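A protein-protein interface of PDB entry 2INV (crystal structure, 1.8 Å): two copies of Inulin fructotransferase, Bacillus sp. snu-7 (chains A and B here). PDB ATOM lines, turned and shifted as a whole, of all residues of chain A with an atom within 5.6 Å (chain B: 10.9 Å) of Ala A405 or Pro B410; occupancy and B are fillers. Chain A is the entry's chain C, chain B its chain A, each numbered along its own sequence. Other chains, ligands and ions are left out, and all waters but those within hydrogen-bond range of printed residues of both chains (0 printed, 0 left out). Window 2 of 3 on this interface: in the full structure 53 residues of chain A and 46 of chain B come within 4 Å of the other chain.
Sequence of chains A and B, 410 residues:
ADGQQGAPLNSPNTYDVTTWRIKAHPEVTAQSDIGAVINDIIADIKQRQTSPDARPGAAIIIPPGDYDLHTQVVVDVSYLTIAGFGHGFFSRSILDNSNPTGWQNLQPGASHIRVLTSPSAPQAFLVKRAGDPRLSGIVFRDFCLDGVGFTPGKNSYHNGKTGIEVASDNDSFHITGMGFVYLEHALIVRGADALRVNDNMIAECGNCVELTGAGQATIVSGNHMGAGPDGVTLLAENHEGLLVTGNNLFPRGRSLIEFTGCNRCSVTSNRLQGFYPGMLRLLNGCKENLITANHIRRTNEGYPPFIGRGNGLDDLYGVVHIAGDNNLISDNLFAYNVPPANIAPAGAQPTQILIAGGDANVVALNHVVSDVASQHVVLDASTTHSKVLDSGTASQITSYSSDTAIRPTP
OD2 of Asp B390 lies within salt-bridge range of NH2 of Arg A407.
The chain-end carboxylate of Pro B410 is in salt-bridge range of the side-chain amino group of Lys A387, at 3.0 Å.
The side-chain carboxylate (OD2) of Asp B390 is in salt-bridge range of the guanidinium group (NH2) of Arg B407.
O of Asp B390 sits at hydrogen-bond distance from N of Asn B366, at 3.3 Å.
N of Ser B391 is in hydrogen-bond range of OG1 of Thr B409, 3.3 Å away.
O of Val A388 lies within hydrogen-bond range of N of Arg A407.
N of Gly B392 sits at hydrogen-bond distance from OG1 of Thr B409 (2.7 Å).
The backbone NH of Ala A405 lies within hydrogen-bond range of the backbone carbonyl oxygen of Ser A386, at 3.0 Å.
CG2 of Thr B409 touches CD of Lys A387, at 3.5 Å.
CD1 of Leu A389 touches CG of Asp B390, 3.9 Å away.
Pro B410 touches Leu A389.
CB of Ala A405 touches OXT of Pro B410 (3.9 Å).
NH1 of Arg A407 touches NE of Arg B407, 3.5 Å away.
NH1 of Arg A407 touches CD of Pro B410 (3.8 Å).
Of the printed residues of chain B, Ala A405 touches Pro B410 (3.9 Å).
No residue of chain B comes within 4 Å of Val A388.
No residue of chain B comes within 4 Å of Thr A404.
No residue of chain B comes within 4 Å of Ile A406.
Printed residues of chain B within 4 Å of Leu A389: Asp B390 and Pro B410.
Of the printed residues of chain A, Asp B390 touches Leu A389 (3.9 Å) and Arg A407 (2.8 Å).
Of the printed residues of chain A, Arg B407 touches Arg A407.
Ser B391 touches none of the printed residues of chain A.
The nearest residue of chain A that does not touch Pro B410 is Ile A406 (5.4 Å).
The nearest printed residue of chain B that does not touch Arg A407 is Pro B408 (4.4 Å).
Of the 19 printed residues of chain B, 4 touch a printed residue of chain A.
Hydrophobic or aromatic side chains of chain B within 4 Å of the printed part of chain A: Pro B410.
Among the printed residues, Asp or Glu carboxylates within 4 Å of a Lys or Arg side-chain nitrogen of the other chain: Arg A407 with Asp B390.
Arg A407 touches its own counterpart, Arg B407.
4 positions are printed for both chains.
Of the 8 pairs that touch across the chains among the printed residues, 1 has its exchanged pair printed and touching as well.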
ATOM      1  N   SER A 386     -13.104 -13.779  24.389  1.00  0.00           N
ATOM      2  CA  SER A 386     -12.896 -13.099  23.105  1.00  0.00           C
ATOM      3  C   SER A 386     -14.242 -12.895  22.403  1.00  0.00           C
ATOM      4  O   SER A 386     -15.228 -13.551  22.738  1.00  0.00           O
ATOM      5  CB  SER A 386     -11.989 -13.932  22.190  1.00  0.00           C
ATOM      6  OG  SER A 386     -10.729 -14.179  22.789  1.00  0.00           O
ATOM      7  N   LYS A 387     -14.274 -11.989  21.428  1.00  0.00           N
ATOM      8  CA  LYS A 387     -15.496 -11.702  20.668  1.00  0.00           C
ATOM      9  C   LYS A 387     -15.158 -11.517  19.194  1.00  0.00           C
ATOM     10  O   LYS A 387     -14.311 -10.691  18.851  1.00  0.00           O
ATOM     11  CB  LYS A 387     -16.159 -10.411  21.162  1.00  0.00           C
ATOM     12  CG  LYS A 387     -16.593 -10.406  22.613  1.00  0.00           C
ATOM     13  CD  LYS A 387     -17.811  -9.544  22.840  1.00  0.00           C
ATOM     14  CE  LYS A 387     -18.177  -9.519  24.310  1.00  0.00           C
ATOM     15  NZ  LYS A 387     -18.717 -10.820  24.743  1.00  0.00           N
ATOM     16  N   VAL A 388     -15.821 -12.268  18.323  1.00  0.00           N
ATOM     17  CA  VAL A 388     -15.571 -12.130  16.900  1.00  0.00           C
ATOM     18  C   VAL A 388     -16.872 -11.803  16.184  1.00  0.00           C
ATOM     19  O   VAL A 388     -17.815 -12.606  16.166  1.00  0.00           O
ATOM     20  CB  VAL A 388     -14.944 -13.408  16.309  1.00  0.00           C
ATOM     21  CG1 VAL A 388     -14.548 -13.173  14.860  1.00  0.00           C
ATOM     22  CG2 VAL A 388     -13.727 -13.810  17.130  1.00  0.00           C
ATOM     23  N   LEU A 389     -16.906 -10.604  15.603  1.00  0.00           N
ATOM     24  CA  LEU A 389     -18.083 -10.117  14.894  1.00  0.00           C
ATOM     25  C   LEU A 389     -17.781  -9.745  13.455  1.00  0.00           C
ATOM     26  O   LEU A 389     -16.787  -9.060  13.173  1.00  0.00           O
ATOM     27  CB  LEU A 389     -18.633  -8.850  15.541  1.00  0.00           C
ATOM     28  CG  LEU A 389     -18.735  -8.657  17.046  1.00  0.00           C
ATOM     29  CD1 LEU A 389     -19.201  -7.232  17.316  1.00  0.00           C
ATOM     30  CD2 LEU A 389     -19.707  -9.648  17.627  1.00  0.00           C
ATOM     31  N   ASP A 403     -15.512 -19.704  25.642  1.00  0.00           N
ATOM     32  CA  ASP A 403     -16.242 -18.523  26.075  1.00  0.00           C
ATOM     33  C   ASP A 403     -16.211 -17.485  24.965  1.00  0.00           C
ATOM     34  O   ASP A 403     -16.594 -16.330  25.168  1.00  0.00           O
ATOM     35  CB  ASP A 403     -15.659 -17.928  27.357  1.00  0.00           C
ATOM     36  CG  ASP A 403     -14.176 -18.184  27.500  1.00  0.00           C
ATOM     37  OD1 ASP A 403     -13.404 -17.828  26.583  1.00  0.00           O
ATOM     38  OD2 ASP A 403     -13.777 -18.740  28.548  1.00  0.00           O
ATOM     39  N   THR A 404     -15.761 -17.898  23.785  1.00  0.00           N
ATOM     40  CA  THR A 404     -15.707 -16.976  22.671  1.00  0.00           C
ATOM     41  C   THR A 404     -17.108 -16.720  22.148  1.00  0.00           C
ATOM     42  O   THR A 404     -17.909 -17.648  21.995  1.00  0.00           O
ATOM     43  CB  THR A 404     -14.855 -17.518  21.515  1.00  0.00           C
ATOM     44  OG1 THR A 404     -13.486 -17.614  21.930  1.00  0.00           O
ATOM     45  CG2 THR A 404     -14.959 -16.584  20.316  1.00  0.00           C
ATOM     46  N   ALA A 405     -17.405 -15.451  21.894  1.00  0.00           N
ATOM     47  CA  ALA A 405     -18.694 -15.067  21.348  1.00  0.00           C
ATOM     48  C   ALA A 405     -18.430 -14.745  19.884  1.00  0.00           C
ATOM     49  O   ALA A 405     -17.594 -13.888  19.570  1.00  0.00           O
ATOM     50  CB  ALA A 405     -19.232 -13.854  22.075  1.00  0.00           C
ATOM     51  N   ILE A 406     -19.137 -15.442  18.998  1.00  0.00           N
ATOM     52  CA  ILE A 406     -18.956 -15.270  17.563  1.00  0.00           C
ATOM     53  C   ILE A 406     -20.260 -14.936  16.846  1.00  0.00           C
ATOM     54  O   ILE A 406     -21.309 -15.501  17.155  1.00  0.00           O
ATOM     55  CB  ILE A 406     -18.409 -16.568  16.923  1.00  0.00           C
ATOM     56  CG1 ILE A 406     -17.142 -17.024  17.650  1.00  0.00           C
ATOM     57  CG2 ILE A 406     -18.130 -16.353  15.441  1.00  0.00           C
ATOM     58  CD1 ILE A 406     -16.622 -18.368  17.190  1.00  0.00           C
ATOM     59  N   ARG A 407     -20.190 -14.014  15.888  1.00  0.00           N
ATOM     60  CA  ARG A 407     -21.354 -13.648  15.082  1.00  0.00           C
ATOM     61  C   ARG A 407     -20.953 -13.701  13.620  1.00  0.00           C
ATOM     62  O   ARG A 407     -20.092 -12.944  13.180  1.00  0.00           O
ATOM     63  CB  ARG A 407     -21.868 -12.251  15.413  1.00  0.00           C
ATOM     64  CG  ARG A 407     -23.000 -11.827  14.465  1.00  0.00           C
ATOM     65  CD  ARG A 407     -23.621 -10.505  14.872  1.00  0.00           C
ATOM     66  NE  ARG A 407     -22.793  -9.368  14.482  1.00  0.00           N
ATOM     67  CZ  ARG A 407     -22.740  -8.228  15.163  1.00  0.00           C
ATOM     68  NH1 ARG A 407     -23.463  -8.080  16.265  1.00  0.00           N
ATOM     69  NH2 ARG A 407     -21.969  -7.239  14.744  1.00  0.00           N
ATOM     70  N   LEU B 365     -20.043  -0.187  17.335  1.00  0.00           N
ATOM     71  CA  LEU B 365     -18.708  -0.754  17.513  1.00  0.00           C
ATOM     72  C   LEU B 365     -17.752   0.115  18.323  1.00  0.00           C
ATOM     73  O   LEU B 365     -16.798   0.689  17.788  1.00  0.00           O
ATOM     74  CB  LEU B 365     -18.083  -1.081  16.156  1.00  0.00           C
ATOM     75  CG  LEU B 365     -16.820  -1.942  16.232  1.00  0.00           C
ATOM     76  CD1 LEU B 365     -17.123  -3.225  16.994  1.00  0.00           C
ATOM     77  CD2 LEU B 365     -16.326  -2.258  14.832  1.00  0.00           C
ATOM     78  N   ASN B 366     -18.022   0.198  19.621  1.00  0.00           N
ATOM     79  CA  ASN B 366     -17.209   0.960  20.559  1.00  0.00           C
ATOM     80  C   ASN B 366     -16.851   0.013  21.697  1.00  0.00           C
ATOM     81  O   ASN B 366     -17.729  -0.434  22.447  1.00  0.00           O
ATOM     82  CB  ASN B 366     -18.001   2.156  21.095  1.00  0.00           C
ATOM     83  CG  ASN B 366     -18.201   3.234  20.053  1.00  0.00           C
ATOM     84  OD1 ASN B 366     -17.269   3.974  19.717  1.00  0.00           O
ATOM     85  ND2 ASN B 366     -19.416   3.324  19.521  1.00  0.00           N
ATOM     86  N   HIS B 367     -15.563  -0.290  21.819  1.00  0.00           N
ATOM     87  CA  HIS B 367     -15.089  -1.193  22.853  1.00  0.00           C
ATOM     88  C   HIS B 367     -14.729  -0.450  24.134  1.00  0.00           C
ATOM     89  O   HIS B 367     -13.882   0.448  24.125  1.00  0.00           O
ATOM     90  CB  HIS B 367     -13.876  -1.979  22.355  1.00  0.00           C
ATOM     91  CG  HIS B 367     -13.400  -3.024  23.316  1.00  0.00           C
ATOM     92  ND1 HIS B 367     -12.067  -3.223  23.603  1.00  0.00           N
ATOM     93  CD2 HIS B 367     -14.080  -3.946  24.043  1.00  0.00           C
ATOM     94  CE1 HIS B 367     -11.944  -4.217  24.463  1.00  0.00           C
ATOM     95  NE2 HIS B 367     -13.150  -4.674  24.745  1.00  0.00           N
ATOM     96  N   HIS B 376     -21.647   2.011  29.178  1.00  0.00           N
ATOM     97  CA  HIS B 376     -20.965   2.308  27.929  1.00  0.00           C
ATOM     98  C   HIS B 376     -21.670   3.405  27.155  1.00  0.00           C
ATOM     99  O   HIS B 376     -21.033   4.267  26.545  1.00  0.00           O
ATOM    100  CB  HIS B 376     -20.897   1.050  27.069  1.00  0.00           C
ATOM    101  CG  HIS B 376     -20.102  -0.054  27.680  1.00  0.00           C
ATOM    102  ND1 HIS B 376     -19.690  -1.157  26.966  1.00  0.00           N
ATOM    103  CD2 HIS B 376     -19.644  -0.229  28.944  1.00  0.00           C
ATOM    104  CE1 HIS B 376     -19.013  -1.965  27.761  1.00  0.00           C
ATOM    105  NE2 HIS B 376     -18.970  -1.425  28.966  1.00  0.00           N
ATOM    106  N   VAL B 388     -27.941   2.083  18.896  1.00  0.00           N
ATOM    107  CA  VAL B 388     -26.753   1.607  19.590  1.00  0.00           C
ATOM    108  C   VAL B 388     -26.479   0.162  19.199  1.00  0.00           C
ATOM    109  O   VAL B 388     -27.267  -0.744  19.509  1.00  0.00           O
ATOM    110  CB  VAL B 388     -26.907   1.725  21.118  1.00  0.00           C
ATOM    111  CG1 VAL B 388     -25.601   1.364  21.806  1.00  0.00           C
ATOM    112  CG2 VAL B 388     -27.317   3.143  21.483  1.00  0.00           C
ATOM    113  N   LEU B 389     -25.360  -0.029  18.502  1.00  0.00           N
ATOM    114  CA  LEU B 389     -24.954  -1.344  18.022  1.00  0.00           C
ATOM    115  C   LEU B 389     -23.577  -1.735  18.522  1.00  0.00           C
ATOM    116  O   LEU B 389     -22.644  -0.918  18.519  1.00  0.00           O
ATOM    117  CB  LEU B 389     -24.866  -1.371  16.500  1.00  0.00           C
ATOM    118  CG  LEU B 389     -25.876  -0.678  15.599  1.00  0.00           C
ATOM    119  CD1 LEU B 389     -25.422  -0.824  14.152  1.00  0.00           C
ATOM    120  CD2 LEU B 389     -27.234  -1.289  15.793  1.00  0.00           C
ATOM    121  N   ASP B 390     -23.443  -2.993  18.921  1.00  0.00           N
ATOM    122  CA  ASP B 390     -22.159  -3.516  19.354  1.00  0.00           C
ATOM    123  C   ASP B 390     -21.315  -2.548  20.175  1.00  0.00           C
ATOM    124  O   ASP B 390     -20.142  -2.324  19.876  1.00  0.00           O
ATOM    125  CB  ASP B 390     -21.398  -3.975  18.114  1.00  0.00           C
ATOM    126  CG  ASP B 390     -22.263  -4.829  17.205  1.00  0.00           C
ATOM    127  OD1 ASP B 390     -23.054  -5.636  17.741  1.00  0.00           O
ATOM    128  OD2 ASP B 390     -22.158  -4.708  15.965  1.00  0.00           O
ATOM    129  N   SER B 391     -21.915  -1.988  21.219  1.00  0.00           N
ATOM    130  CA  SER B 391     -21.208  -1.057  22.089  1.00  0.00           C
ATOM    131  C   SER B 391     -21.445  -1.428  23.549  1.00  0.00           C
ATOM    132  O   SER B 391     -21.311  -0.590  24.448  1.00  0.00           O
ATOM    133  CB  SER B 391     -21.665   0.381  21.823  1.00  0.00           C
ATOM    134  OG  SER B 391     -21.297   0.788  20.519  1.00  0.00           O
ATOM    135  N   GLY B 392     -21.798  -2.692  23.781  1.00  0.00           N
ATOM    136  CA  GLY B 392     -22.035  -3.156  25.137  1.00  0.00           C
ATOM    137  C   GLY B 392     -23.234  -4.078  25.271  1.00  0.00           C
ATOM    138  O   GLY B 392     -24.096  -4.136  24.383  1.00  0.00           O
ATOM    139  N   THR B 393     -23.300  -4.801  26.386  1.00  0.00           N
ATOM    140  CA  THR B 393     -24.418  -5.704  26.631  1.00  0.00           C
ATOM    141  C   THR B 393     -25.580  -4.824  27.050  1.00  0.00           C
ATOM    142  O   THR B 393     -25.387  -3.649  27.347  1.00  0.00           O
ATOM    143  CB  THR B 393     -24.104  -6.709  27.761  1.00  0.00           C
ATOM    144  OG1 THR B 393     -22.877  -7.387  27.469  1.00  0.00           O
ATOM    145  CG2 THR B 393     -25.228  -7.728  27.897  1.00  0.00           C
ATOM    146  N   ALA B 394     -26.779  -5.386  27.078  1.00  0.00           N
ATOM    147  CA  ALA B 394     -27.948  -4.618  27.458  1.00  0.00           C
ATOM    148  C   ALA B 394     -27.819  -3.973  28.835  1.00  0.00           C
ATOM    149  O   ALA B 394     -28.448  -2.942  29.097  1.00  0.00           O
ATOM    150  CB  ALA B 394     -29.185  -5.498  27.413  1.00  0.00           C
ATOM    151  N   SER B 395     -27.016  -4.555  29.721  1.00  0.00           N
ATOM    152  CA  SER B 395     -26.884  -3.972  31.053  1.00  0.00           C
ATOM    153  C   SER B 395     -25.760  -2.946  31.156  1.00  0.00           C
ATOM    154  O   SER B 395     -25.531  -2.368  32.219  1.00  0.00           O
ATOM    155  CB  SER B 395     -26.704  -5.071  32.103  1.00  0.00           C
ATOM    156  OG  SER B 395     -25.479  -5.780  31.940  1.00  0.00           O
ATOM    157  N   GLN B 396     -25.072  -2.709  30.045  1.00  0.00           N
ATOM    158  CA  GLN B 396     -24.008  -1.717  30.016  1.00  0.00           C
ATOM    159  C   GLN B 396     -24.532  -0.537  29.200  1.00  0.00           C
ATOM    160  O   GLN B 396     -23.793   0.413  28.908  1.00  0.00           O
ATOM    161  CB  GLN B 396     -22.744  -2.300  29.373  1.00  0.00           C
ATOM    162  CG  GLN B 396     -22.169  -3.529  30.136  1.00  0.00           C
ATOM    163  CD  GLN B 396     -20.991  -4.188  29.442  1.00  0.00           C
ATOM    164  OE1 GLN B 396     -21.027  -4.458  28.233  1.00  0.00           O
ATOM    165  NE2 GLN B 396     -19.939  -4.466  30.213  1.00  0.00           N
ATOM    166  N   ILE B 397     -25.825  -0.598  28.873  1.00  0.00           N
ATOM    167  CA  ILE B 397     -26.499   0.438  28.083  1.00  0.00           C
ATOM    168  C   ILE B 397     -27.783   0.962  28.746  1.00  0.00           C
ATOM    169  O   ILE B 397     -28.694   0.182  29.055  1.00  0.00           O
ATOM    170  CB  ILE B 397     -26.886  -0.104  26.692  1.00  0.00           C
ATOM    171  CG1 ILE B 397     -25.641  -0.612  25.967  1.00  0.00           C
ATOM    172  CG2 ILE B 397     -27.580   0.975  25.884  1.00  0.00           C
ATOM    173  CD1 ILE B 397     -25.922  -1.216  24.604  1.00  0.00           C
ATOM    174  N   ILE B 406     -31.485  -0.878  20.021  1.00  0.00           N
ATOM    175  CA  ILE B 406     -30.251  -1.399  20.590  1.00  0.00           C
ATOM    176  C   ILE B 406     -29.968  -2.836  20.163  1.00  0.00           C
ATOM    177  O   ILE B 406     -30.882  -3.653  20.071  1.00  0.00           O
ATOM    178  CB  ILE B 406     -30.319  -1.391  22.136  1.00  0.00           C
ATOM    179  CG1 ILE B 406     -30.628   0.016  22.650  1.00  0.00           C
ATOM    180  CG2 ILE B 406     -29.009  -1.907  22.728  1.00  0.00           C
ATOM    181  CD1 ILE B 406     -30.810   0.089  24.153  1.00  0.00           C
ATOM    182  N   ARG B 407     -28.696  -3.136  19.905  1.00  0.00           N
ATOM    183  CA  ARG B 407     -28.277  -4.490  19.546  1.00  0.00           C
ATOM    184  C   ARG B 407     -27.082  -4.867  20.402  1.00  0.00           C
ATOM    185  O   ARG B 407     -26.018  -4.262  20.296  1.00  0.00           O
ATOM    186  CB  ARG B 407     -27.893  -4.609  18.075  1.00  0.00           C
ATOM    187  CG  ARG B 407     -27.339  -6.006  17.747  1.00  0.00           C
ATOM    188  CD  ARG B 407     -27.035  -6.178  16.271  1.00  0.00           C
ATOM    189  NE  ARG B 407     -25.805  -5.495  15.878  1.00  0.00           N
ATOM    190  CZ  ARG B 407     -25.599  -4.990  14.668  1.00  0.00           C
ATOM    191  NH1 ARG B 407     -26.543  -5.088  13.739  1.00  0.00           N
ATOM    192  NH2 ARG B 407     -24.451  -4.395  14.379  1.00  0.00           N
ATOM    193  N   PRO B 408     -27.265  -5.849  21.293  1.00  0.00           N
ATOM    194  CA  PRO B 408     -26.197  -6.310  22.181  1.00  0.00           C
ATOM    195  C   PRO B 408     -24.890  -6.712  21.515  1.00  0.00           C
ATOM    196  O   PRO B 408     -24.875  -7.202  20.389  1.00  0.00           O
ATOM    197  CB  PRO B 408     -26.820  -7.511  22.864  1.00  0.00           C
ATOM    198  CG  PRO B 408     -28.218  -7.122  23.022  1.00  0.00           C
ATOM    199  CD  PRO B 408     -28.569  -6.392  21.724  1.00  0.00           C
ATOM    200  N   THR B 409     -23.783  -6.472  22.209  1.00  0.00           N
ATOM    201  CA  THR B 409     -22.501  -6.930  21.706  1.00  0.00           C
ATOM    202  C   THR B 409     -22.799  -8.349  22.178  1.00  0.00           C
ATOM    203  O   THR B 409     -23.082  -8.557  23.357  1.00  0.00           O
ATOM    204  CB  THR B 409     -21.304  -6.391  22.504  1.00  0.00           C
ATOM    205  OG1 THR B 409     -21.245  -4.966  22.396  1.00  0.00           O
ATOM    206  CG2 THR B 409     -20.010  -6.977  21.952  1.00  0.00           C
ATOM    207  N   PRO B 410     -22.797  -9.333  21.273  1.00  0.00           N
ATOM    208  CA  PRO B 410     -23.097 -10.693  21.725  1.00  0.00           C
ATOM    209  C   PRO B 410     -22.422 -11.134  23.019  1.00  0.00           C
ATOM    210  O   PRO B 410     -23.025 -11.908  23.797  1.00  0.00           O
ATOM    211  CB  PRO B 410     -22.696 -11.540  20.535  1.00  0.00           C
ATOM    212  CG  PRO B 410     -23.201 -10.676  19.399  1.00  0.00           C
ATOM    213  CD  PRO B 410     -22.785  -9.261  19.801  1.00  0.00           C
ATOM    214  OXT PRO B 410     -21.267 -10.706  23.239  1.00  0.00           O
